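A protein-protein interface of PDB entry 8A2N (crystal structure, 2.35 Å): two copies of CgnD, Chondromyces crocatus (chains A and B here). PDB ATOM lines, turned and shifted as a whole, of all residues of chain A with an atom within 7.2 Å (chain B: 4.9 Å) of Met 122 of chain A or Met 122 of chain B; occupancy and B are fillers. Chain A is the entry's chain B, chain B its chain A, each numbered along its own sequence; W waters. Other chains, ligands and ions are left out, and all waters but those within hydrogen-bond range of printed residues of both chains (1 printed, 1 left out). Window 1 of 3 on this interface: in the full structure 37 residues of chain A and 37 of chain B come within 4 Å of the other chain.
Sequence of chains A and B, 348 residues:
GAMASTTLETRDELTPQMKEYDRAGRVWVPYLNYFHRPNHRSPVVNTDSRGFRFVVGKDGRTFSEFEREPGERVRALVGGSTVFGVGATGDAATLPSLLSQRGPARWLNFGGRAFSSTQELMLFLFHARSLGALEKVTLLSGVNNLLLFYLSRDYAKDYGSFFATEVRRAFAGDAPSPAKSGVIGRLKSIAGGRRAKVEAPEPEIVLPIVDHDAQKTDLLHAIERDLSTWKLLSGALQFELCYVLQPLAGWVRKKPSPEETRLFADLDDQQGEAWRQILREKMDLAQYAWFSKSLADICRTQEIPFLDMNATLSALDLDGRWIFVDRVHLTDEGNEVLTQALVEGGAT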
ATOM      1  N   PRO A  30      19.836 -12.284 -15.138  1.00  0.00           N
ATOM      2  CA  PRO A  30      19.987 -11.865 -13.738  1.00  0.00           C
ATOM      3  C   PRO A  30      18.998 -10.789 -13.360  1.00  0.00           C
ATOM      4  O   PRO A  30      18.677  -9.922 -14.167  1.00  0.00           O
ATOM      5  CB  PRO A  30      21.434 -11.340 -13.671  1.00  0.00           C
ATOM      6  CG  PRO A  30      21.788 -10.989 -15.100  1.00  0.00           C
ATOM      7  CD  PRO A  30      21.037 -11.992 -15.945  1.00  0.00           C
ATOM      8  N   TYR A  31      18.513 -10.876 -12.126  1.00  0.00           N
ATOM      9  CA  TYR A  31      17.597  -9.926 -11.506  1.00  0.00           C
ATOM     10  C   TYR A  31      16.195 -10.124 -12.025  1.00  0.00           C
ATOM     11  O   TYR A  31      15.290 -10.374 -11.226  1.00  0.00           O
ATOM     12  CB  TYR A  31      18.048  -8.493 -11.710  1.00  0.00           C
ATOM     13  CG  TYR A  31      19.485  -8.265 -11.292  1.00  0.00           C
ATOM     14  CD1 TYR A  31      19.869  -8.393  -9.973  1.00  0.00           C
ATOM     15  CD2 TYR A  31      20.454  -7.920 -12.234  1.00  0.00           C
ATOM     16  CE1 TYR A  31      21.185  -8.193  -9.587  1.00  0.00           C
ATOM     17  CE2 TYR A  31      21.775  -7.724 -11.861  1.00  0.00           C
ATOM     18  CZ  TYR A  31      22.133  -7.854 -10.531  1.00  0.00           C
ATOM     19  OH  TYR A  31      23.453  -7.662 -10.108  1.00  0.00           O
ATOM     20  N   LEU A  32      15.997 -10.015 -13.343  1.00  0.00           N
ATOM     21  CA  LEU A  32      14.698 -10.352 -13.915  1.00  0.00           C
ATOM     22  C   LEU A  32      14.384 -11.835 -13.760  1.00  0.00           C
ATOM     23  O   LEU A  32      13.209 -12.216 -13.780  1.00  0.00           O
ATOM     24  CB  LEU A  32      14.657  -9.992 -15.398  1.00  0.00           C
ATOM     25  CG  LEU A  32      14.394  -8.563 -15.810  1.00  0.00           C
ATOM     26  CD1 LEU A  32      14.121  -8.539 -17.291  1.00  0.00           C
ATOM     27  CD2 LEU A  32      13.226  -7.994 -15.044  1.00  0.00           C
ATOM     28  N   ASN A  33      15.421 -12.675 -13.673  1.00  0.00           N
ATOM     29  CA  ASN A  33      15.318 -14.128 -13.605  1.00  0.00           C
ATOM     30  C   ASN A  33      15.061 -14.775 -14.954  1.00  0.00           C
ATOM     31  O   ASN A  33      15.622 -15.832 -15.228  1.00  0.00           O
ATOM     32  CB  ASN A  33      14.246 -14.548 -12.612  1.00  0.00           C
ATOM     33  CG  ASN A  33      14.528 -14.021 -11.227  1.00  0.00           C
ATOM     34  OD1 ASN A  33      13.690 -13.324 -10.635  1.00  0.00           O
ATOM     35  ND2 ASN A  33      15.721 -14.288 -10.724  1.00  0.00           N
ATOM     36  N   PHE A 110       6.556  -3.835 -24.288  1.00  0.00           N
ATOM     37  CA  PHE A 110       7.220  -4.193 -23.035  1.00  0.00           C
ATOM     38  C   PHE A 110       6.405  -5.242 -22.291  1.00  0.00           C
ATOM     39  O   PHE A 110       6.237  -5.159 -21.063  1.00  0.00           O
ATOM     40  CB  PHE A 110       7.423  -2.953 -22.158  1.00  0.00           C
ATOM     41  CG  PHE A 110       8.775  -2.368 -22.256  1.00  0.00           C
ATOM     42  CD1 PHE A 110       9.700  -2.506 -21.196  1.00  0.00           C
ATOM     43  CD2 PHE A 110       9.151  -1.676 -23.390  1.00  0.00           C
ATOM     44  CE1 PHE A 110      10.928  -1.973 -21.287  1.00  0.00           C
ATOM     45  CE2 PHE A 110      10.429  -1.128 -23.497  1.00  0.00           C
ATOM     46  CZ  PHE A 110      11.335  -1.294 -22.446  1.00  0.00           C
ATOM     47  N   PHE A 115       5.381 -12.304 -16.544  1.00  0.00           N
ATOM     48  CA  PHE A 115       5.956 -11.370 -15.590  1.00  0.00           C
ATOM     49  C   PHE A 115       4.992 -10.999 -14.474  1.00  0.00           C
ATOM     50  O   PHE A 115       3.791 -10.851 -14.692  1.00  0.00           O
ATOM     51  CB  PHE A 115       6.393 -10.066 -16.239  1.00  0.00           C
ATOM     52  CG  PHE A 115       7.751 -10.088 -16.832  1.00  0.00           C
ATOM     53  CD1 PHE A 115       8.533 -11.220 -16.807  1.00  0.00           C
ATOM     54  CD2 PHE A 115       8.292  -8.913 -17.301  1.00  0.00           C
ATOM     55  CE1 PHE A 115       9.808 -11.201 -17.325  1.00  0.00           C
ATOM     56  CE2 PHE A 115       9.579  -8.899 -17.805  1.00  0.00           C
ATOM     57  CZ  PHE A 115      10.319 -10.054 -17.814  1.00  0.00           C
ATOM     58  N   SER A 116       5.569 -10.791 -13.291  1.00  0.00           N
ATOM     59  CA  SER A 116       4.965 -10.136 -12.145  1.00  0.00           C
ATOM     60  C   SER A 116       5.070  -8.624 -12.295  1.00  0.00           C
ATOM     61  O   SER A 116       5.806  -8.099 -13.143  1.00  0.00           O
ATOM     62  CB  SER A 116       5.674 -10.552 -10.859  1.00  0.00           C
ATOM     63  OG  SER A 116       7.021 -10.098 -10.869  1.00  0.00           O
ATOM     64  N   SER A 117       4.385  -7.912 -11.403  1.00  0.00           N
ATOM     65  CA  SER A 117       4.463  -6.458 -11.446  1.00  0.00           C
ATOM     66  C   SER A 117       5.904  -6.002 -11.277  1.00  0.00           C
ATOM     67  O   SER A 117       6.360  -5.091 -11.976  1.00  0.00           O
ATOM     68  CB  SER A 117       3.568  -5.846 -10.383  1.00  0.00           C
ATOM     69  OG  SER A 117       4.016  -6.199  -9.073  1.00  0.00           O
ATOM     70  N   THR A 118       6.649  -6.657 -10.395  1.00  0.00           N
ATOM     71  CA  THR A 118       8.024  -6.260 -10.120  1.00  0.00           C
ATOM     72  C   THR A 118       8.920  -6.486 -11.327  1.00  0.00           C
ATOM     73  O   THR A 118       9.716  -5.607 -11.675  1.00  0.00           O
ATOM     74  CB  THR A 118       8.561  -7.011  -8.911  1.00  0.00           C
ATOM     75  OG1 THR A 118       7.761  -6.701  -7.776  1.00  0.00           O
ATOM     76  CG2 THR A 118      10.024  -6.615  -8.609  1.00  0.00           C
ATOM     77  N   GLN A 119       8.796  -7.649 -11.990  1.00  0.00           N
ATOM     78  CA  GLN A 119       9.572  -7.879 -13.200  1.00  0.00           C
ATOM     79  C   GLN A 119       9.262  -6.844 -14.274  1.00  0.00           C
ATOM     80  O   GLN A 119      10.161  -6.403 -14.987  1.00  0.00           O
ATOM     81  CB  GLN A 119       9.303  -9.266 -13.741  1.00  0.00           C
ATOM     82  CG  GLN A 119       9.812 -10.398 -12.811  1.00  0.00           C
ATOM     83  CD  GLN A 119       9.431 -11.773 -13.344  1.00  0.00           C
ATOM     84  OE1 GLN A 119       8.256 -12.074 -13.537  1.00  0.00           O
ATOM     85  NE2 GLN A 119      10.415 -12.593 -13.601  1.00  0.00           N
ATOM     86  N   GLU A 120       8.000  -6.471 -14.427  1.00  0.00           N
ATOM     87  CA  GLU A 120       7.621  -5.454 -15.404  1.00  0.00           C
ATOM     88  C   GLU A 120       8.330  -4.141 -15.115  1.00  0.00           C
ATOM     89  O   GLU A 120       8.856  -3.507 -16.028  1.00  0.00           O
ATOM     90  CB  GLU A 120       6.100  -5.215 -15.377  1.00  0.00           C
ATOM     91  CG  GLU A 120       5.227  -6.438 -15.592  1.00  0.00           C
ATOM     92  CD  GLU A 120       3.749  -6.200 -15.193  1.00  0.00           C
ATOM     93  OE1 GLU A 120       3.439  -5.272 -14.383  1.00  0.00           O
ATOM     94  OE2 GLU A 120       2.878  -6.968 -15.671  1.00  0.00           O
ATOM     95  N   LEU A 121       8.357  -3.724 -13.836  1.00  0.00           N
ATOM     96  CA  LEU A 121       9.017  -2.485 -13.463  1.00  0.00           C
ATOM     97  C   LEU A 121      10.518  -2.567 -13.717  1.00  0.00           C
ATOM     98  O   LEU A 121      11.119  -1.615 -14.225  1.00  0.00           O
ATOM     99  CB  LEU A 121       8.753  -2.163 -12.004  1.00  0.00           C
ATOM    100  CG  LEU A 121       9.516  -0.988 -11.415  1.00  0.00           C
ATOM    101  CD1 LEU A 121       9.071   0.310 -12.062  1.00  0.00           C
ATOM    102  CD2 LEU A 121       9.335  -0.943  -9.889  1.00  0.00           C
ATOM    103  N   MET A 122      11.134  -3.698 -13.398  1.00  0.00           N
ATOM    104  CA  MET A 122      12.580  -3.836 -13.565  1.00  0.00           C
ATOM    105  C   MET A 122      12.978  -3.876 -15.022  1.00  0.00           C
ATOM    106  O   MET A 122      13.963  -3.266 -15.420  1.00  0.00           O
ATOM    107  CB  MET A 122      13.071  -5.080 -12.868  1.00  0.00           C
ATOM    108  CG  MET A 122      12.959  -5.019 -11.351  1.00  0.00           C
ATOM    109  SD  MET A 122      13.481  -6.593 -10.579  1.00  0.00           S
ATOM    110  CE  MET A 122      15.106  -6.744 -11.255  1.00  0.00           C
ATOM    111  N   LEU A 123      12.215  -4.582 -15.844  1.00  0.00           N
ATOM    112  CA  LEU A 123      12.463  -4.553 -17.273  1.00  0.00           C
ATOM    113  C   LEU A 123      12.505  -3.116 -17.777  1.00  0.00           C
ATOM    114  O   LEU A 123      13.377  -2.751 -18.576  1.00  0.00           O
ATOM    115  CB  LEU A 123      11.397  -5.357 -17.997  1.00  0.00           C
ATOM    116  CG  LEU A 123      11.687  -5.585 -19.487  1.00  0.00           C
ATOM    117  CD1 LEU A 123      12.850  -6.528 -19.703  1.00  0.00           C
ATOM    118  CD2 LEU A 123      10.427  -6.101 -20.165  1.00  0.00           C
ATOM    119  N   PHE A 124      11.565  -2.290 -17.317  1.00  0.00           N
ATOM    120  CA  PHE A 124      11.536  -0.883 -17.728  1.00  0.00           C
ATOM    121  C   PHE A 124      12.713  -0.119 -17.169  1.00  0.00           C
ATOM    122  O   PHE A 124      13.343   0.657 -17.889  1.00  0.00           O
ATOM    123  CB  PHE A 124      10.226  -0.238 -17.289  1.00  0.00           C
ATOM    124  CG  PHE A 124      10.074   1.166 -17.700  1.00  0.00           C
ATOM    125  CD1 PHE A 124       9.467   1.480 -18.905  1.00  0.00           C
ATOM    126  CD2 PHE A 124      10.515   2.198 -16.879  1.00  0.00           C
ATOM    127  CE1 PHE A 124       9.301   2.812 -19.308  1.00  0.00           C
ATOM    128  CE2 PHE A 124      10.375   3.537 -17.281  1.00  0.00           C
ATOM    129  CZ  PHE A 124       9.758   3.838 -18.497  1.00  0.00           C
ATOM    130  N   LEU A 125      13.036  -0.317 -15.902  1.00  0.00           N
ATOM    131  CA  LEU A 125      14.181   0.400 -15.335  1.00  0.00           C
ATOM    132  C   LEU A 125      15.490  -0.013 -15.997  1.00  0.00           C
ATOM    133  O   LEU A 125      16.419   0.784 -16.091  1.00  0.00           O
ATOM    134  CB  LEU A 125      14.277   0.127 -13.831  1.00  0.00           C
ATOM    135  CG  LEU A 125      13.201   0.770 -12.969  1.00  0.00           C
ATOM    136  CD1 LEU A 125      13.193   0.111 -11.578  1.00  0.00           C
ATOM    137  CD2 LEU A 125      13.427   2.252 -12.867  1.00  0.00           C
ATOM    138  N   PHE A 126      15.581  -1.250 -16.479  1.00  0.00           N
ATOM    139  CA  PHE A 126      16.806  -1.678 -17.130  1.00  0.00           C
ATOM    140  C   PHE A 126      16.967  -1.071 -18.522  1.00  0.00           C
ATOM    141  O   PHE A 126      18.084  -0.961 -19.013  1.00  0.00           O
ATOM    142  CB  PHE A 126      16.840  -3.200 -17.244  1.00  0.00           C
ATOM    143  CG  PHE A 126      17.223  -3.894 -15.986  1.00  0.00           C
ATOM    144  CD1 PHE A 126      18.412  -3.672 -15.407  1.00  0.00           C
ATOM    145  CD2 PHE A 126      16.381  -4.805 -15.433  1.00  0.00           C
ATOM    146  CE1 PHE A 126      18.768  -4.343 -14.245  1.00  0.00           C
ATOM    147  CE2 PHE A 126      16.717  -5.469 -14.283  1.00  0.00           C
ATOM    148  CZ  PHE A 126      17.882  -5.227 -13.682  1.00  0.00           C
ATOM    149  N   HIS A 127      15.878  -0.689 -19.172  1.00  0.00           N
ATOM    150  CA  HIS A 127      15.953  -0.262 -20.561  1.00  0.00           C
ATOM    151  C   HIS A 127      15.445   1.161 -20.783  1.00  0.00           C
ATOM    152  O   HIS A 127      15.546   1.664 -21.895  1.00  0.00           O
ATOM    153  CB  HIS A 127      15.192  -1.259 -21.459  1.00  0.00           C
ATOM    154  CG  HIS A 127      15.771  -2.641 -21.445  1.00  0.00           C
ATOM    155  ND1 HIS A 127      16.927  -2.980 -22.121  1.00  0.00           N
ATOM    156  CD2 HIS A 127      15.363  -3.774 -20.820  1.00  0.00           C
ATOM    157  CE1 HIS A 127      17.215  -4.251 -21.907  1.00  0.00           C
ATOM    158  NE2 HIS A 127      16.274  -4.760 -21.124  1.00  0.00           N
ATOM    159  N   ALA A 128      14.955   1.838 -19.746  1.00  0.00           N
ATOM    160  CA  ALA A 128      14.294   3.118 -19.959  1.00  0.00           C
ATOM    161  C   ALA A 128      15.214   4.102 -20.671  1.00  0.00           C
ATOM    162  O   ALA A 128      14.804   4.787 -21.605  1.00  0.00           O
ATOM    163  CB  ALA A 128      13.831   3.704 -18.638  1.00  0.00           C
ATOM    164  N   TYR A 159       9.277  -8.182  -1.210  1.00  0.00           N
ATOM    165  CA  TYR A 159       9.871  -8.430  -2.523  1.00  0.00           C
ATOM    166  C   TYR A 159       8.919  -9.105  -3.489  1.00  0.00           C
ATOM    167  O   TYR A 159       8.847  -8.710  -4.659  1.00  0.00           O
ATOM    168  CB  TYR A 159      11.129  -9.295  -2.358  1.00  0.00           C
ATOM    169  CG  TYR A 159      12.122  -8.638  -1.459  1.00  0.00           C
ATOM    170  CD1 TYR A 159      12.942  -7.636  -1.935  1.00  0.00           C
ATOM    171  CD2 TYR A 159      12.231  -8.997  -0.125  1.00  0.00           C
ATOM    172  CE1 TYR A 159      13.877  -7.015  -1.113  1.00  0.00           C
ATOM    173  CE2 TYR A 159      13.153  -8.400   0.704  1.00  0.00           C
ATOM    174  CZ  TYR A 159      13.973  -7.393   0.199  1.00  0.00           C
ATOM    175  OH  TYR A 159      14.885  -6.770   0.998  1.00  0.00           O
ATOM    176  N   TRP A 230       6.460   3.460 -10.212  1.00  0.00           N
ATOM    177  CA  TRP A 230       5.941   3.947 -11.491  1.00  0.00           C
ATOM    178  C   TRP A 230       5.479   5.427 -11.416  1.00  0.00           C
ATOM    179  O   TRP A 230       5.784   6.248 -12.304  1.00  0.00           O
ATOM    180  CB  TRP A 230       4.772   3.094 -11.948  1.00  0.00           C
ATOM    181  CG  TRP A 230       5.171   1.837 -12.659  1.00  0.00           C
ATOM    182  CD1 TRP A 230       4.944   0.533 -12.247  1.00  0.00           C
ATOM    183  CD2 TRP A 230       5.853   1.748 -13.918  1.00  0.00           C
ATOM    184  NE1 TRP A 230       5.457  -0.349 -13.186  1.00  0.00           N
ATOM    185  CE2 TRP A 230       5.994   0.382 -14.227  1.00  0.00           C
ATOM    186  CE3 TRP A 230       6.320   2.677 -14.805  1.00  0.00           C
ATOM    187  CZ2 TRP A 230       6.581  -0.051 -15.411  1.00  0.00           C
ATOM    188  CZ3 TRP A 230       6.916   2.252 -15.962  1.00  0.00           C
ATOM    189  CH2 TRP A 230       7.059   0.898 -16.240  1.00  0.00           C
ATOM    190  N   TYR B  31      14.731 -11.453  -6.877  1.00  0.00           N
ATOM    191  CA  TYR B  31      15.172 -10.251  -7.566  1.00  0.00           C
ATOM    192  C   TYR B  31      16.499  -9.776  -7.022  1.00  0.00           C
ATOM    193  O   TYR B  31      17.463  -9.676  -7.777  1.00  0.00           O
ATOM    194  CB  TYR B  31      14.118  -9.158  -7.488  1.00  0.00           C
ATOM    195  CG  TYR B  31      12.749  -9.636  -7.904  1.00  0.00           C
ATOM    196  CD1 TYR B  31      12.518 -10.046  -9.193  1.00  0.00           C
ATOM    197  CD2 TYR B  31      11.700  -9.715  -6.984  1.00  0.00           C
ATOM    198  CE1 TYR B  31      11.254 -10.475  -9.588  1.00  0.00           C
ATOM    199  CE2 TYR B  31      10.471 -10.164  -7.353  1.00  0.00           C
ATOM    200  CZ  TYR B  31      10.239 -10.543  -8.671  1.00  0.00           C
ATOM    201  OH  TYR B  31       9.012 -11.002  -9.087  1.00  0.00           O
ATOM    202  N   LEU B  32      16.570  -9.456  -5.737  1.00  0.00           N
ATOM    203  CA  LEU B  32      17.860  -9.111  -5.148  1.00  0.00           C
ATOM    204  C   LEU B  32      18.826 -10.295  -5.204  1.00  0.00           C
ATOM    205  O   LEU B  32      20.033 -10.105  -5.237  1.00  0.00           O
ATOM    206  CB  LEU B  32      17.689  -8.666  -3.703  1.00  0.00           C
ATOM    207  CG  LEU B  32      17.418  -7.208  -3.374  1.00  0.00           C
ATOM    208  CD1 LEU B  32      17.444  -7.049  -1.810  1.00  0.00           C
ATOM    209  CD2 LEU B  32      18.381  -6.261  -4.006  1.00  0.00           C
ATOM    210  N   THR B 118      23.646  -2.741  -9.245  1.00  0.00           N
ATOM    211  CA  THR B 118      22.245  -2.971  -9.537  1.00  0.00           C
ATOM    212  C   THR B 118      21.495  -3.444  -8.295  1.00  0.00           C
ATOM    213  O   THR B 118      20.334  -3.080  -8.096  1.00  0.00           O
ATOM    214  CB  THR B 118      22.109  -3.984 -10.670  1.00  0.00           C
ATOM    215  OG1 THR B 118      22.787  -3.499 -11.822  1.00  0.00           O
ATOM    216  CG2 THR B 118      20.669  -4.233 -11.020  1.00  0.00           C
ATOM    217  N   GLN B 119      22.133  -4.256  -7.454  1.00  0.00           N
ATOM    218  CA  GLN B 119      21.502  -4.640  -6.210  1.00  0.00           C
ATOM    219  C   GLN B 119      21.389  -3.463  -5.265  1.00  0.00           C
ATOM    220  O   GLN B 119      20.453  -3.411  -4.467  1.00  0.00           O
ATOM    221  CB  GLN B 119      22.283  -5.768  -5.520  1.00  0.00           C
ATOM    222  CG  GLN B 119      22.395  -7.068  -6.324  1.00  0.00           C
ATOM    223  CD  GLN B 119      23.325  -8.064  -5.652  1.00  0.00           C
ATOM    224  OE1 GLN B 119      24.546  -7.845  -5.568  1.00  0.00           O
ATOM    225  NE2 GLN B 119      22.759  -9.140  -5.136  1.00  0.00           N
ATOM    226  N   GLU B 120      22.364  -2.554  -5.278  1.00  0.00           N
ATOM    227  CA  GLU B 120      22.258  -1.366  -4.446  1.00  0.00           C
ATOM    228  C   GLU B 120      21.012  -0.576  -4.831  1.00  0.00           C
ATOM    229  O   GLU B 120      20.250  -0.134  -3.971  1.00  0.00           O
ATOM    230  CB  GLU B 120      23.487  -0.475  -4.592  1.00  0.00           C
ATOM    231  CG  GLU B 120      24.748  -0.971  -3.885  1.00  0.00           C
ATOM    232  CD  GLU B 120      26.039  -0.323  -4.467  1.00  0.00           C
ATOM    233  OE1 GLU B 120      25.949   0.645  -5.285  1.00  0.00           O
ATOM    234  OE2 GLU B 120      27.161  -0.772  -4.102  1.00  0.00           O
ATOM    235  N   LEU B 121      20.818  -0.370  -6.139  1.00  0.00           N
ATOM    236  CA  LEU B 121      19.686   0.405  -6.610  1.00  0.00           C
ATOM    237  C   LEU B 121      18.380  -0.285  -6.270  1.00  0.00           C
ATOM    238  O   LEU B 121      17.437   0.363  -5.807  1.00  0.00           O
ATOM    239  CB  LEU B 121      19.798   0.624  -8.110  1.00  0.00           C
ATOM    240  CG  LEU B 121      18.615   1.270  -8.800  1.00  0.00           C
ATOM    241  CD1 LEU B 121      18.412   2.664  -8.221  1.00  0.00           C
ATOM    242  CD2 LEU B 121      18.801   1.312 -10.302  1.00  0.00           C
ATOM    243  N   MET B 122      18.322  -1.614  -6.470  1.00  0.00           N
ATOM    244  CA  MET B 122      17.086  -2.337  -6.240  1.00  0.00           C
ATOM    245  C   MET B 122      16.725  -2.365  -4.776  1.00  0.00           C
ATOM    246  O   MET B 122      15.549  -2.202  -4.407  1.00  0.00           O
ATOM    247  CB  MET B 122      17.209  -3.747  -6.792  1.00  0.00           C
ATOM    248  CG  MET B 122      17.164  -3.832  -8.300  1.00  0.00           C
ATOM    249  SD  MET B 122      17.544  -5.544  -8.781  1.00  0.00           S
ATOM    250  CE  MET B 122      15.991  -6.286  -8.281  1.00  0.00           C
ATOM    251  N   LEU B 123      17.712  -2.577  -3.912  1.00  0.00           N
ATOM    252  CA  LEU B 123      17.446  -2.548  -2.479  1.00  0.00           C
ATOM    253  C   LEU B 123      16.795  -1.235  -2.109  1.00  0.00           C
ATOM    254  O   LEU B 123      15.843  -1.203  -1.337  1.00  0.00           O
ATOM    255  CB  LEU B 123      18.732  -2.755  -1.692  1.00  0.00           C
ATOM    256  CG  LEU B 123      18.575  -2.834  -0.174  1.00  0.00           C
ATOM    257  CD1 LEU B 123      17.913  -4.127   0.259  1.00  0.00           C
ATOM    258  CD2 LEU B 123      19.951  -2.676   0.468  1.00  0.00           C
ATOM    259  N   PHE B 124      17.292  -0.129  -2.670  1.00  0.00           N
ATOM    260  CA  PHE B 124      16.698   1.176  -2.372  1.00  0.00           C
ATOM    261  C   PHE B 124      15.292   1.293  -2.945  1.00  0.00           C
ATOM    262  O   PHE B 124      14.372   1.787  -2.282  1.00  0.00           O
ATOM    263  CB  PHE B 124      17.599   2.281  -2.918  1.00  0.00           C
ATOM    264  CG  PHE B 124      17.114   3.655  -2.625  1.00  0.00           C
ATOM    265  CD1 PHE B 124      17.397   4.253  -1.414  1.00  0.00           C
ATOM    266  CD2 PHE B 124      16.357   4.363  -3.575  1.00  0.00           C
ATOM    267  CE1 PHE B 124      16.915   5.527  -1.132  1.00  0.00           C
ATOM    268  CE2 PHE B 124      15.889   5.638  -3.301  1.00  0.00           C
ATOM    269  CZ  PHE B 124      16.149   6.219  -2.092  1.00  0.00           C
ATOM    270  N   LEU B 125      15.089   0.856  -4.179  1.00  0.00           N
ATOM    271  CA  LEU B 125      13.742   0.945  -4.767  1.00  0.00           C
ATOM    272  C   LEU B 125      12.734   0.097  -4.003  1.00  0.00           C
ATOM    273  O   LEU B 125      11.572   0.496  -3.851  1.00  0.00           O
ATOM    274  CB  LEU B 125      13.765   0.515  -6.220  1.00  0.00           C
ATOM    275  CG  LEU B 125      14.361   1.531  -7.190  1.00  0.00           C
ATOM    276  CD1 LEU B 125      14.625   0.880  -8.536  1.00  0.00           C
ATOM    277  CD2 LEU B 125      13.451   2.709  -7.380  1.00  0.00           C
ATOM    278  N   PHE B 126      13.158  -1.054  -3.475  1.00  0.00           N
ATOM    279  CA  PHE B 126      12.228  -1.920  -2.744  1.00  0.00           C
ATOM    280  C   PHE B 126      11.774  -1.321  -1.415  1.00  0.00           C
ATOM    281  O   PHE B 126      10.683  -1.659  -0.937  1.00  0.00           O
ATOM    282  CB  PHE B 126      12.852  -3.279  -2.472  1.00  0.00           C
ATOM    283  CG  PHE B 126      12.767  -4.221  -3.621  1.00  0.00           C
ATOM    284  CD1 PHE B 126      11.557  -4.620  -4.106  1.00  0.00           C
ATOM    285  CD2 PHE B 126      13.916  -4.741  -4.199  1.00  0.00           C
ATOM    286  CE1 PHE B 126      11.476  -5.522  -5.173  1.00  0.00           C
ATOM    287  CE2 PHE B 126      13.834  -5.614  -5.277  1.00  0.00           C
ATOM    288  CZ  PHE B 126      12.611  -5.984  -5.766  1.00  0.00           C
HETATM  289  O   HOH W   1      15.708 -13.499  -7.758  1.00  0.00           O
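The side-chain hydroxyl (OG) of Ser 116 of chain A is in hydrogen-bond range of the side-chain hydroxyl (OH) of Tyr 31 of chain B, at 2.8 Å.
Tyr 31 of chain A touches Thr 118 of chain B, and with the chains exchanged Thr 118 of chain A touches Tyr 31 of chain B. Tyr 31 of chain A touches Gln 119 of chain B, and with the chains exchanged Gln 119 of chain A touches Tyr 31 of chain B. Met 122 of chain B touches its own counterpart, Met 122 of chain A. Leu 125 of chain B touches its own counterpart, Leu 125 of chain A. Positions printed for both chains: 31, 32, 118, 119, 120, 121, 122, 123, 124, 125 and 126. Of the 16 pairs that touch across the chains among the printed residues, 11 have their exchanged pair printed and touching as well.
Printed residues of chain B that touch a printed residue of chain A: Tyr 31, Leu 32, Thr 118, Gln 119, Met 122, Leu 125 and Phe 126. Hydrophobic or aromatic side chains of chain B within 4 Å of the printed part of chain A: Tyr 31, Leu 32, Met 122, Leu 125 and Phe 126. Along chain B the printed residues that touch a printed residue of chain A span positions 31 to 126. Among the printed residues, no Asp or Glu carboxylate lies within 4 Å of a Lys or Arg side-chain nitrogen of the other chain.
Tyr 31 of chain B touches Tyr 31 of chain A. Tyr 31 of chain A touches Met 122 of chain B (CD1 to SD, 3.9 Å). CD1 of Tyr 31 of chain B touches OD1 of Asn 33 of chain A, at 3.8 Å. CG of Gln 119 of chain A touches CE1 of Tyr 31 of chain B (3.5 Å). Tyr 31 of chain B touches Met 122 of chain A (CD1 to SD, 3.8 Å). Met 122 of chain A touches Met 122 of chain B. CD1 of Leu 125 of chain A touches CD1 of Leu 125 of chain B, at 3.4 Å. CE1 of Phe 126 of chain A touches CG2 of Thr 118 of chain B, at 3.7 Å. Tyr 159 of chain A touches Tyr 31 of chain B. CE1 of Tyr 159 of chain A touches CD1 of Leu 32 of chain B, 3.6 Å away.
The backbone carbonyl oxygen (O) of Tyr 31 of chain A sits close to the side-chain amide oxygen (OD1) of Asn 33 of chain A (3.4 Å). O of Leu 32 of chain A sits at hydrogen-bond distance from NE2 of Gln 119 of chain A, at 2.8 Å. OG of Ser 116 of chain A lies close to N of Thr 118 of chain A (3.5 Å). The backbone NH (N) of Ser 116 of chain A is in hydrogen-bond range of the side-chain amide oxygen (OE1) of Gln 119 of chain A. The side-chain amide nitrogen of Gln 119 of chain B lies within hydrogen-bond range of the backbone carbonyl oxygen of Leu 32 of chain B, 2.9 Å away.
Met 122 of chain A touches two residues of chain B. Printed residues of chain A within 4 Å of Leu 32 of chain B: Tyr 159. Printed residues of chain B within 4 Å of Phe 126 of chain A: Thr 118 (3.7 Å). Of the printed residues of chain B, Ser 116 of chain A touches Tyr 31. Of the printed residues of chain B, Gln 119 of chain A touches Tyr 31. Printed residues of chain B within 4 Å of Tyr 31 of chain A: Tyr 31 (3.5 Å), Thr 118 (3.8 Å), Gln 119 (3.7 Å) and Met 122 (3.9 Å). Phe 115 of chain A touches none of the printed residues of chain B. Phe 124 of chain B touches none of the printed residues of chain A. The nearest printed residue of chain B that does not touch Met 122 of chain A is Phe 126 of chain B (4.9 Å).
Water W1 lies within hydrogen-bond range of N of Tyr 31 of chain B (2.4 Å) and ND2 of Asn 33 of chain A (3.1 Å).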
